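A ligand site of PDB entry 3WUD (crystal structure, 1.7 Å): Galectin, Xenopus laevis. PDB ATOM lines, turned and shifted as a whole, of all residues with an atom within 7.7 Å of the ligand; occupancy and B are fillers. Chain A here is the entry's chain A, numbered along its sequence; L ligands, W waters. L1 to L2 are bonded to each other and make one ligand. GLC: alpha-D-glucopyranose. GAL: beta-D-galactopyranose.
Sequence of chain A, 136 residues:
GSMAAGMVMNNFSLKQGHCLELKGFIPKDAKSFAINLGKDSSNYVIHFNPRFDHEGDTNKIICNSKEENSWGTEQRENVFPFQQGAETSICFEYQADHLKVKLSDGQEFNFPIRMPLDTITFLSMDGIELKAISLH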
ATOM      1  N   SER A  32      16.166  16.093  -6.205  1.00  0.00           N
ATOM      2  CA  SER A  32      15.208  14.995  -6.416  1.00  0.00           C
ATOM      3  C   SER A  32      13.931  15.582  -7.094  1.00  0.00           C
ATOM      4  O   SER A  32      13.770  16.818  -7.172  1.00  0.00           O
ATOM      5  CB  SER A  32      14.799  14.345  -5.067  1.00  0.00           C
ATOM      6  OG  SER A  32      14.160  15.279  -4.273  1.00  0.00           O
ATOM      7  N   PHE A  33      13.078  14.758  -7.582  1.00  0.00           N
ATOM      8  CA  PHE A  33      11.732  15.199  -7.984  1.00  0.00           C
ATOM      9  C   PHE A  33      10.735  14.040  -7.662  1.00  0.00           C
ATOM     10  O   PHE A  33      11.170  12.900  -7.415  1.00  0.00           O
ATOM     11  CB  PHE A  33      11.690  15.601  -9.475  1.00  0.00           C
ATOM     12  CG  PHE A  33      11.913  14.464 -10.454  1.00  0.00           C
ATOM     13  CD1 PHE A  33      10.837  13.806 -11.045  1.00  0.00           C
ATOM     14  CD2 PHE A  33      13.201  14.089 -10.868  1.00  0.00           C
ATOM     15  CE1 PHE A  33      11.014  12.778 -11.942  1.00  0.00           C
ATOM     16  CE2 PHE A  33      13.396  13.084 -11.798  1.00  0.00           C
ATOM     17  CZ  PHE A  33      12.308  12.426 -12.326  1.00  0.00           C
ATOM     18  N   ALA A  34       9.430  14.340  -7.583  1.00  0.00           N
ATOM     19  CA  ALA A  34       8.492  13.279  -7.197  1.00  0.00           C
ATOM     20  C   ALA A  34       7.275  13.444  -8.069  1.00  0.00           C
ATOM     21  O   ALA A  34       6.869  14.600  -8.353  1.00  0.00           O
ATOM     22  CB  ALA A  34       8.124  13.355  -5.703  1.00  0.00           C
ATOM     23  N   ASN A  36       3.419  11.817  -7.831  1.00  0.00           N
ATOM     24  CA  ASN A  36       2.454  11.085  -7.060  1.00  0.00           C
ATOM     25  C   ASN A  36       1.170  10.773  -7.826  1.00  0.00           C
ATOM     26  O   ASN A  36       0.641  11.661  -8.443  1.00  0.00           O
ATOM     27  CB  ASN A  36       2.119  11.967  -5.904  1.00  0.00           C
ATOM     28  CG  ASN A  36       3.314  12.288  -5.043  1.00  0.00           C
ATOM     29  OD1 ASN A  36       4.066  11.390  -4.644  1.00  0.00           O
ATOM     30  ND2 ASN A  36       3.490  13.546  -4.756  1.00  0.00           N
ATOM     31  N   HIS A  47       4.197   7.071  -4.894  1.00  0.00           N
ATOM     32  CA  HIS A  47       5.057   8.192  -4.755  1.00  0.00           C
ATOM     33  C   HIS A  47       6.324   7.707  -5.416  1.00  0.00           C
ATOM     34  O   HIS A  47       6.962   6.752  -4.913  1.00  0.00           O
ATOM     35  CB  HIS A  47       5.279   8.533  -3.281  1.00  0.00           C
ATOM     36  CG  HIS A  47       6.398   9.517  -3.010  1.00  0.00           C
ATOM     37  ND1 HIS A  47       6.292  10.870  -3.236  1.00  0.00           N
ATOM     38  CD2 HIS A  47       7.605   9.308  -2.457  1.00  0.00           C
ATOM     39  CE1 HIS A  47       7.407  11.460  -2.811  1.00  0.00           C
ATOM     40  NE2 HIS A  47       8.182  10.537  -2.281  1.00  0.00           N
ATOM     41  N   PHE A  48       6.647   8.308  -6.549  1.00  0.00           N
ATOM     42  CA  PHE A  48       7.740   7.954  -7.428  1.00  0.00           C
ATOM     43  C   PHE A  48       8.795   9.049  -7.321  1.00  0.00           C
ATOM     44  O   PHE A  48       8.543  10.195  -7.705  1.00  0.00           O
ATOM     45  CB  PHE A  48       7.214   7.891  -8.860  1.00  0.00           C
ATOM     46  CG  PHE A  48       8.262   7.628  -9.888  1.00  0.00           C
ATOM     47  CD1 PHE A  48       8.694   6.325 -10.136  1.00  0.00           C
ATOM     48  CD2 PHE A  48       8.814   8.672 -10.617  1.00  0.00           C
ATOM     49  CE1 PHE A  48       9.645   6.074 -11.096  1.00  0.00           C
ATOM     50  CE2 PHE A  48       9.808   8.443 -11.588  1.00  0.00           C
ATOM     51  CZ  PHE A  48      10.231   7.126 -11.791  1.00  0.00           C
ATOM     52  N   ASN A  49       9.900   8.769  -6.631  1.00  0.00           N
ATOM     53  CA  ASN A  49      10.851   9.785  -6.217  1.00  0.00           C
ATOM     54  C   ASN A  49      12.372   9.518  -6.597  1.00  0.00           C
ATOM     55  O   ASN A  49      13.111   9.000  -5.776  1.00  0.00           O
ATOM     56  CB  ASN A  49      10.715   9.911  -4.695  1.00  0.00           C
ATOM     57  CG  ASN A  49      11.525  11.063  -4.077  1.00  0.00           C
ATOM     58  OD1 ASN A  49      11.906  10.954  -2.927  1.00  0.00           O
ATOM     59  ND2 ASN A  49      11.752  12.144  -4.800  1.00  0.00           N
ATOM     60  N   ARG A  51      15.992  10.358  -6.886  1.00  0.00           N
ATOM     61  CA  ARG A  51      16.802  11.099  -6.028  1.00  0.00           C
ATOM     62  C   ARG A  51      18.234  11.134  -6.608  1.00  0.00           C
ATOM     63  O   ARG A  51      18.908  10.068  -6.689  1.00  0.00           O
ATOM     64  CB  ARG A  51      16.887  10.438  -4.654  1.00  0.00           C
ATOM     65  CG  ARG A  51      15.538  10.414  -3.951  1.00  0.00           C
ATOM     66  CD  ARG A  51      15.620   9.884  -2.528  1.00  0.00           C
ATOM     67  NE  ARG A  51      14.288   9.937  -1.875  1.00  0.00           N
ATOM     68  CZ  ARG A  51      14.026   9.366  -0.691  1.00  0.00           C
ATOM     69  NH1 ARG A  51      14.988   8.776  -0.012  1.00  0.00           N
ATOM     70  NH2 ARG A  51      12.822   9.457  -0.141  1.00  0.00           N
ATOM     71  N   HIS A  54      19.509  12.981  -2.186  1.00  0.00           N
ATOM     72  CA  HIS A  54      18.454  13.351  -1.274  1.00  0.00           C
ATOM     73  C   HIS A  54      18.254  12.266  -0.277  1.00  0.00           C
ATOM     74  O   HIS A  54      18.294  11.109  -0.593  1.00  0.00           O
ATOM     75  CB  HIS A  54      17.171  13.681  -2.090  1.00  0.00           C
ATOM     76  CG  HIS A  54      16.013  14.055  -1.234  1.00  0.00           C
ATOM     77  ND1 HIS A  54      16.020  15.140  -0.389  1.00  0.00           N
ATOM     78  CD2 HIS A  54      14.787  13.488  -1.126  1.00  0.00           C
ATOM     79  CE1 HIS A  54      14.863  15.191   0.261  1.00  0.00           C
ATOM     80  NE2 HIS A  54      14.088  14.227  -0.196  1.00  0.00           N
ATOM     81  N   GLU A  55      18.112  12.646   0.971  1.00  0.00           N
ATOM     82  CA  GLU A  55      17.953  11.673   2.075  1.00  0.00           C
ATOM     83  C   GLU A  55      19.041  10.611   2.082  1.00  0.00           C
ATOM     84  O   GLU A  55      18.747   9.501   2.422  1.00  0.00           O
ATOM     85  CB  GLU A  55      16.554  11.004   2.050  1.00  0.00           C
ATOM     86  CG  GLU A  55      15.387  11.976   2.082  1.00  0.00           C
ATOM     87  CD  GLU A  55      15.060  12.510   3.474  1.00  0.00           C
ATOM     88  OE1 GLU A  55      14.036  13.232   3.612  1.00  0.00           O
ATOM     89  OE2 GLU A  55      15.772  12.176   4.430  1.00  0.00           O
ATOM     90  N   GLY A  56      20.283  10.957   1.720  1.00  0.00           N
ATOM     91  CA  GLY A  56      21.414   9.998   1.611  1.00  0.00           C
ATOM     92  C   GLY A  56      21.450   9.044   0.415  1.00  0.00           C
ATOM     93  O   GLY A  56      22.373   8.161   0.294  1.00  0.00           O
ATOM     94  N   ASP A  57      20.499   9.223  -0.517  1.00  0.00           N
ATOM     95  CA  ASP A  57      20.369   8.369  -1.691  1.00  0.00           C
ATOM     96  C   ASP A  57      20.936   9.152  -2.899  1.00  0.00           C
ATOM     97  O   ASP A  57      20.643  10.365  -3.005  1.00  0.00           O
ATOM     98  CB  ASP A  57      18.906   7.999  -1.961  1.00  0.00           C
ATOM     99  CG  ASP A  57      18.342   7.148  -0.877  1.00  0.00           C
ATOM    100  OD1 ASP A  57      19.021   6.212  -0.430  1.00  0.00           O
ATOM    101  OD2 ASP A  57      17.235   7.485  -0.441  1.00  0.00           O
ATOM    102  N   ILE A  62      13.336   6.054  -5.244  1.00  0.00           N
ATOM    103  CA  ILE A  62      12.646   5.517  -4.051  1.00  0.00           C
ATOM    104  C   ILE A  62      11.170   5.577  -4.415  1.00  0.00           C
ATOM    105  O   ILE A  62      10.720   6.601  -4.926  1.00  0.00           O
ATOM    106  CB  ILE A  62      12.902   6.428  -2.874  1.00  0.00           C
ATOM    107  CG1 ILE A  62      14.281   6.155  -2.283  1.00  0.00           C
ATOM    108  CG2 ILE A  62      11.855   6.198  -1.761  1.00  0.00           C
ATOM    109  CD1 ILE A  62      15.433   5.956  -3.241  1.00  0.00           C
ATOM    110  N   CYS A  63      10.435   4.467  -4.288  1.00  0.00           N
ATOM    111  CA  CYS A  63       8.968   4.518  -4.418  1.00  0.00           C
ATOM    112  C   CYS A  63       8.336   4.155  -3.072  1.00  0.00           C
ATOM    113  O   CYS A  63       8.878   3.366  -2.266  1.00  0.00           O
ATOM    114  CB  CYS A  63       8.503   3.513  -5.441  1.00  0.00           C
ATOM    115  SG  CYS A  63       9.046   3.998  -7.134  1.00  0.00           S
ATOM    116  N   ASN A  64       7.169   4.713  -2.822  1.00  0.00           N
ATOM    117  CA  ASN A  64       6.403   4.337  -1.667  1.00  0.00           C
ATOM    118  C   ASN A  64       4.934   4.619  -1.903  1.00  0.00           C
ATOM    119  O   ASN A  64       4.562   5.213  -2.882  1.00  0.00           O
ATOM    120  CB  ASN A  64       6.879   5.169  -0.460  1.00  0.00           C
ATOM    121  CG  ASN A  64       6.648   4.434   0.879  1.00  0.00           C
ATOM    122  OD1 ASN A  64       5.871   3.550   0.986  1.00  0.00           O
ATOM    123  ND2 ASN A  64       7.257   4.898   1.917  1.00  0.00           N
ATOM    124  N   SER A  65       4.104   4.129  -1.035  1.00  0.00           N
ATOM    125  CA  SER A  65       2.694   4.447  -0.996  1.00  0.00           C
ATOM    126  C   SER A  65       2.415   5.388   0.133  1.00  0.00           C
ATOM    127  O   SER A  65       3.185   5.445   1.117  1.00  0.00           O
ATOM    128  CB  SER A  65       1.870   3.153  -0.783  1.00  0.00           C
ATOM    129  OG  SER A  65       2.200   2.439   0.407  1.00  0.00           O
ATOM    130  N   TRP A  71       3.113   7.130   5.243  1.00  0.00           N
ATOM    131  CA  TRP A  71       3.987   6.380   4.347  1.00  0.00           C
ATOM    132  C   TRP A  71       3.934   4.840   4.585  1.00  0.00           C
ATOM    133  O   TRP A  71       3.958   4.352   5.732  1.00  0.00           O
ATOM    134  CB  TRP A  71       5.451   6.858   4.403  1.00  0.00           C
ATOM    135  CG  TRP A  71       5.661   8.253   3.949  1.00  0.00           C
ATOM    136  CD1 TRP A  71       6.089   9.348   4.724  1.00  0.00           C
ATOM    137  CD2 TRP A  71       5.400   8.775   2.655  1.00  0.00           C
ATOM    138  NE1 TRP A  71       6.112  10.452   3.940  1.00  0.00           N
ATOM    139  CE2 TRP A  71       5.771  10.122   2.660  1.00  0.00           C
ATOM    140  CE3 TRP A  71       5.067   8.185   1.447  1.00  0.00           C
ATOM    141  CZ2 TRP A  71       5.649  10.934   1.518  1.00  0.00           C
ATOM    142  CZ3 TRP A  71       4.977   8.982   0.323  1.00  0.00           C
ATOM    143  CH2 TRP A  71       5.252  10.301   0.341  1.00  0.00           C
ATOM    144  N   GLY A  72       3.937   4.060   3.502  1.00  0.00           N
ATOM    145  CA  GLY A  72       4.159   2.633   3.575  1.00  0.00           C
ATOM    146  C   GLY A  72       5.609   2.208   3.598  1.00  0.00           C
ATOM    147  O   GLY A  72       6.484   2.949   4.042  1.00  0.00           O
ATOM    148  N   THR A  73       5.857   1.009   3.147  1.00  0.00           N
ATOM    149  CA  THR A  73       7.210   0.452   3.010  1.00  0.00           C
ATOM    150  C   THR A  73       7.907   0.932   1.714  1.00  0.00           C
ATOM    151  O   THR A  73       7.353   0.695   0.618  1.00  0.00           O
ATOM    152  CB  THR A  73       7.138  -1.085   3.024  1.00  0.00           C
ATOM    153  OG1 THR A  73       6.564  -1.474   4.289  1.00  0.00           O
ATOM    154  CG2 THR A  73       8.542  -1.734   2.915  1.00  0.00           C
ATOM    155  N   GLU A  74       9.123   1.545   1.813  1.00  0.00           N
ATOM    156  CA  GLU A  74       9.778   1.986   0.601  1.00  0.00           C
ATOM    157  C   GLU A  74      10.250   0.838  -0.278  1.00  0.00           C
ATOM    158  O   GLU A  74      10.674  -0.195   0.248  1.00  0.00           O
ATOM    159  CB  GLU A  74      11.022   2.806   0.931  1.00  0.00           C
ATOM    160  CG  GLU A  74      10.753   4.191   1.441  1.00  0.00           C
ATOM    161  CD  GLU A  74      12.017   4.993   1.808  1.00  0.00           C
ATOM    162  OE1 GLU A  74      13.146   4.512   1.709  1.00  0.00           O
ATOM    163  OE2 GLU A  74      11.858   6.145   2.130  1.00  0.00           O
ATOM    164  N   GLN A  75      10.212   1.082  -1.582  1.00  0.00           N
ATOM    165  CA  GLN A  75      10.819   0.203  -2.599  1.00  0.00           C
ATOM    166  C   GLN A  75      11.958   1.021  -3.276  1.00  0.00           C
ATOM    167  O   GLN A  75      11.762   2.155  -3.723  1.00  0.00           O
ATOM    168  CB  GLN A  75       9.754  -0.288  -3.588  1.00  0.00           C
ATOM    169  CG  GLN A  75      10.268  -1.350  -4.533  1.00  0.00           C
ATOM    170  CD  GLN A  75       9.187  -1.840  -5.472  1.00  0.00           C
ATOM    171  OE1 GLN A  75       8.179  -2.428  -5.025  1.00  0.00           O
ATOM    172  NE2 GLN A  75       9.369  -1.609  -6.756  1.00  0.00           N
ATOM    173  N   ARG A  76      13.166   0.464  -3.250  1.00  0.00           N
ATOM    174  CA  ARG A  76      14.321   1.134  -3.817  1.00  0.00           C
ATOM    175  C   ARG A  76      14.751   0.481  -5.162  1.00  0.00           C
ATOM    176  O   ARG A  76      14.964  -0.750  -5.256  1.00  0.00           O
ATOM    177  CB  ARG A  76      15.482   1.213  -2.818  1.00  0.00           C
ATOM    178  CG  ARG A  76      15.700   2.568  -2.157  1.00  0.00           C
ATOM    179  CD  ARG A  76      16.811   2.612  -1.078  1.00  0.00           C
ATOM    180  NE  ARG A  76      16.750   3.875  -0.294  1.00  0.00           N
ATOM    181  CZ  ARG A  76      15.848   4.134   0.674  1.00  0.00           C
ATOM    182  NH1 ARG A  76      14.979   3.182   1.034  1.00  0.00           N
ATOM    183  NH2 ARG A  76      15.847   5.332   1.323  1.00  0.00           N
ATOM    184  N   ASP A 126       6.424  17.435  -8.040  1.00  0.00           N
ATOM    185  CA  ASP A 126       7.217  18.432  -7.348  1.00  0.00           C
ATOM    186  C   ASP A 126       8.673  18.246  -7.850  1.00  0.00           C
ATOM    187  O   ASP A 126       9.122  17.141  -8.050  1.00  0.00           O
ATOM    188  CB  ASP A 126       7.116  18.210  -5.829  1.00  0.00           C
ATOM    189  CG  ASP A 126       7.765  19.317  -4.995  1.00  0.00           C
ATOM    190  OD1 ASP A 126       7.882  20.528  -5.398  1.00  0.00           O
ATOM    191  OD2 ASP A 126       8.162  18.948  -3.871  1.00  0.00           O
HETATM  192  C1  GLC L   1      14.140   7.341   5.920  1.00  0.00           C
HETATM  193  C2  GLC L   1      14.469   7.287   4.448  1.00  0.00           C
HETATM  194  C3  GLC L   1      13.906   8.377   3.584  1.00  0.00           C
HETATM  195  C4  GLC L   1      12.656   9.063   4.168  1.00  0.00           C
HETATM  196  C5  GLC L   1      12.801   9.433   5.645  1.00  0.00           C
HETATM  197  C6  GLC L   1      11.490   9.746   6.283  1.00  0.00           C
HETATM  198  O1  GLC L   1      15.174   6.884   6.759  1.00  0.00           O
HETATM  199  O2  GLC L   1      15.801   6.997   4.095  1.00  0.00           O
HETATM  200  O3  GLC L   1      13.698   7.772   2.299  1.00  0.00           O
HETATM  201  O4  GLC L   1      12.519  10.220   3.422  1.00  0.00           O
HETATM  202  O5  GLC L   1      13.334   8.396   6.412  1.00  0.00           O
HETATM  203  O6  GLC L   1      11.806  10.117   7.620  1.00  0.00           O
HETATM  204  C1  GAL L   2      11.145  10.365   2.952  1.00  0.00           C
HETATM  205  C2  GAL L   2      10.973  11.716   2.256  1.00  0.00           C
HETATM  206  C3  GAL L   2       9.581  11.915   1.648  1.00  0.00           C
HETATM  207  C4  GAL L   2       9.229  10.664   0.829  1.00  0.00           C
HETATM  208  C5  GAL L   2       9.458   9.409   1.679  1.00  0.00           C
HETATM  209  C6  GAL L   2       9.156   8.095   0.980  1.00  0.00           C
HETATM  210  O2  GAL L   2      11.166  12.755   3.196  1.00  0.00           O
HETATM  211  O3  GAL L   2       9.564  13.137   0.923  1.00  0.00           O
HETATM  212  O4  GAL L   2      10.060  10.606  -0.345  1.00  0.00           O
HETATM  213  O5  GAL L   2      10.812   9.273   2.126  1.00  0.00           O
HETATM  214  O6  GAL L   2       9.359   6.953   1.795  1.00  0.00           O
HETATM  215  O   HOH W   1      11.281  13.217  -1.314  1.00  0.00           O
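CZ2 of Trp 71 touches C4 of GAL L2 (3.7 Å).
Hydrophobic or aromatic side chains within 4 Å of the ligand: His 47 and Trp 71.
Eight residues have an atom within 4 Å of the ligand: His 47, Asn 49, Arg 51, Glu 55, Asn 64, Trp 71, Glu 74 and Arg 76.
The nearest printed residue that does not touch the ligand is Ile 62 (4.3 Å).
The side-chain carboxylate of Glu 74 lies within hydrogen-bond range of an oxygen (O3) of GLC L1 (2.5 Å).
O4 of GAL L2 is in hydrogen-bond range of NE2 of His 47 (2.7 Å).
The guanidinium group (NH1) of Arg 51 lies within hydrogen-bond range of an oxygen (O3) of GLC L1 (2.8 Å).
The side-chain carboxylate (OE1) of Glu 55 is in hydrogen-bond range of an oxygen (O2) of GAL L2 (2.9 Å).
An oxygen (O6) of GAL L2 sits at hydrogen-bond distance from the side-chain amide nitrogen (ND2) of Asn 64.
The side-chain amide oxygen (OD1) of Asn 49 is in hydrogen-bond range of an oxygen (O4) of GAL L2, at 3.2 Å.
NH2 of Arg 76 is in hydrogen-bond range of O2 of GLC L1.
The side-chain carboxylate (OE1) of Glu 74 lies within salt-bridge range of the guanidinium group (NH2) of Arg 76.
The backbone carbonyl oxygen of Asn 64 is in hydrogen-bond range of the backbone NH of His 47.
The guanidinium group (NE) of Arg 51 sits at hydrogen-bond distance from the side-chain amide oxygen (OD1) of Asn 49 (2.8 Å).
NH1 of Arg 51 is in salt-bridge range of OD2 of Asp 57.
ND2 of Asn 64 is in hydrogen-bond range of O of Gly 72 (3.0 Å).
The backbone carbonyl oxygen (O) of Thr 73 lies close to the side-chain amide oxygen (OD1) of Asn 64 (3.2 Å).
ND2 of Asn 49 sits at hydrogen-bond distance from O of Phe 33.
OD2 of Asp 57 lies within salt-bridge range of NH2 of Arg 76.
Water W1 lies within hydrogen-bond range of an oxygen (O3) of GAL L2, the side-chain amide oxygen (OD1) of Asn 49 and a ring nitrogen (NE2) of His 54.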
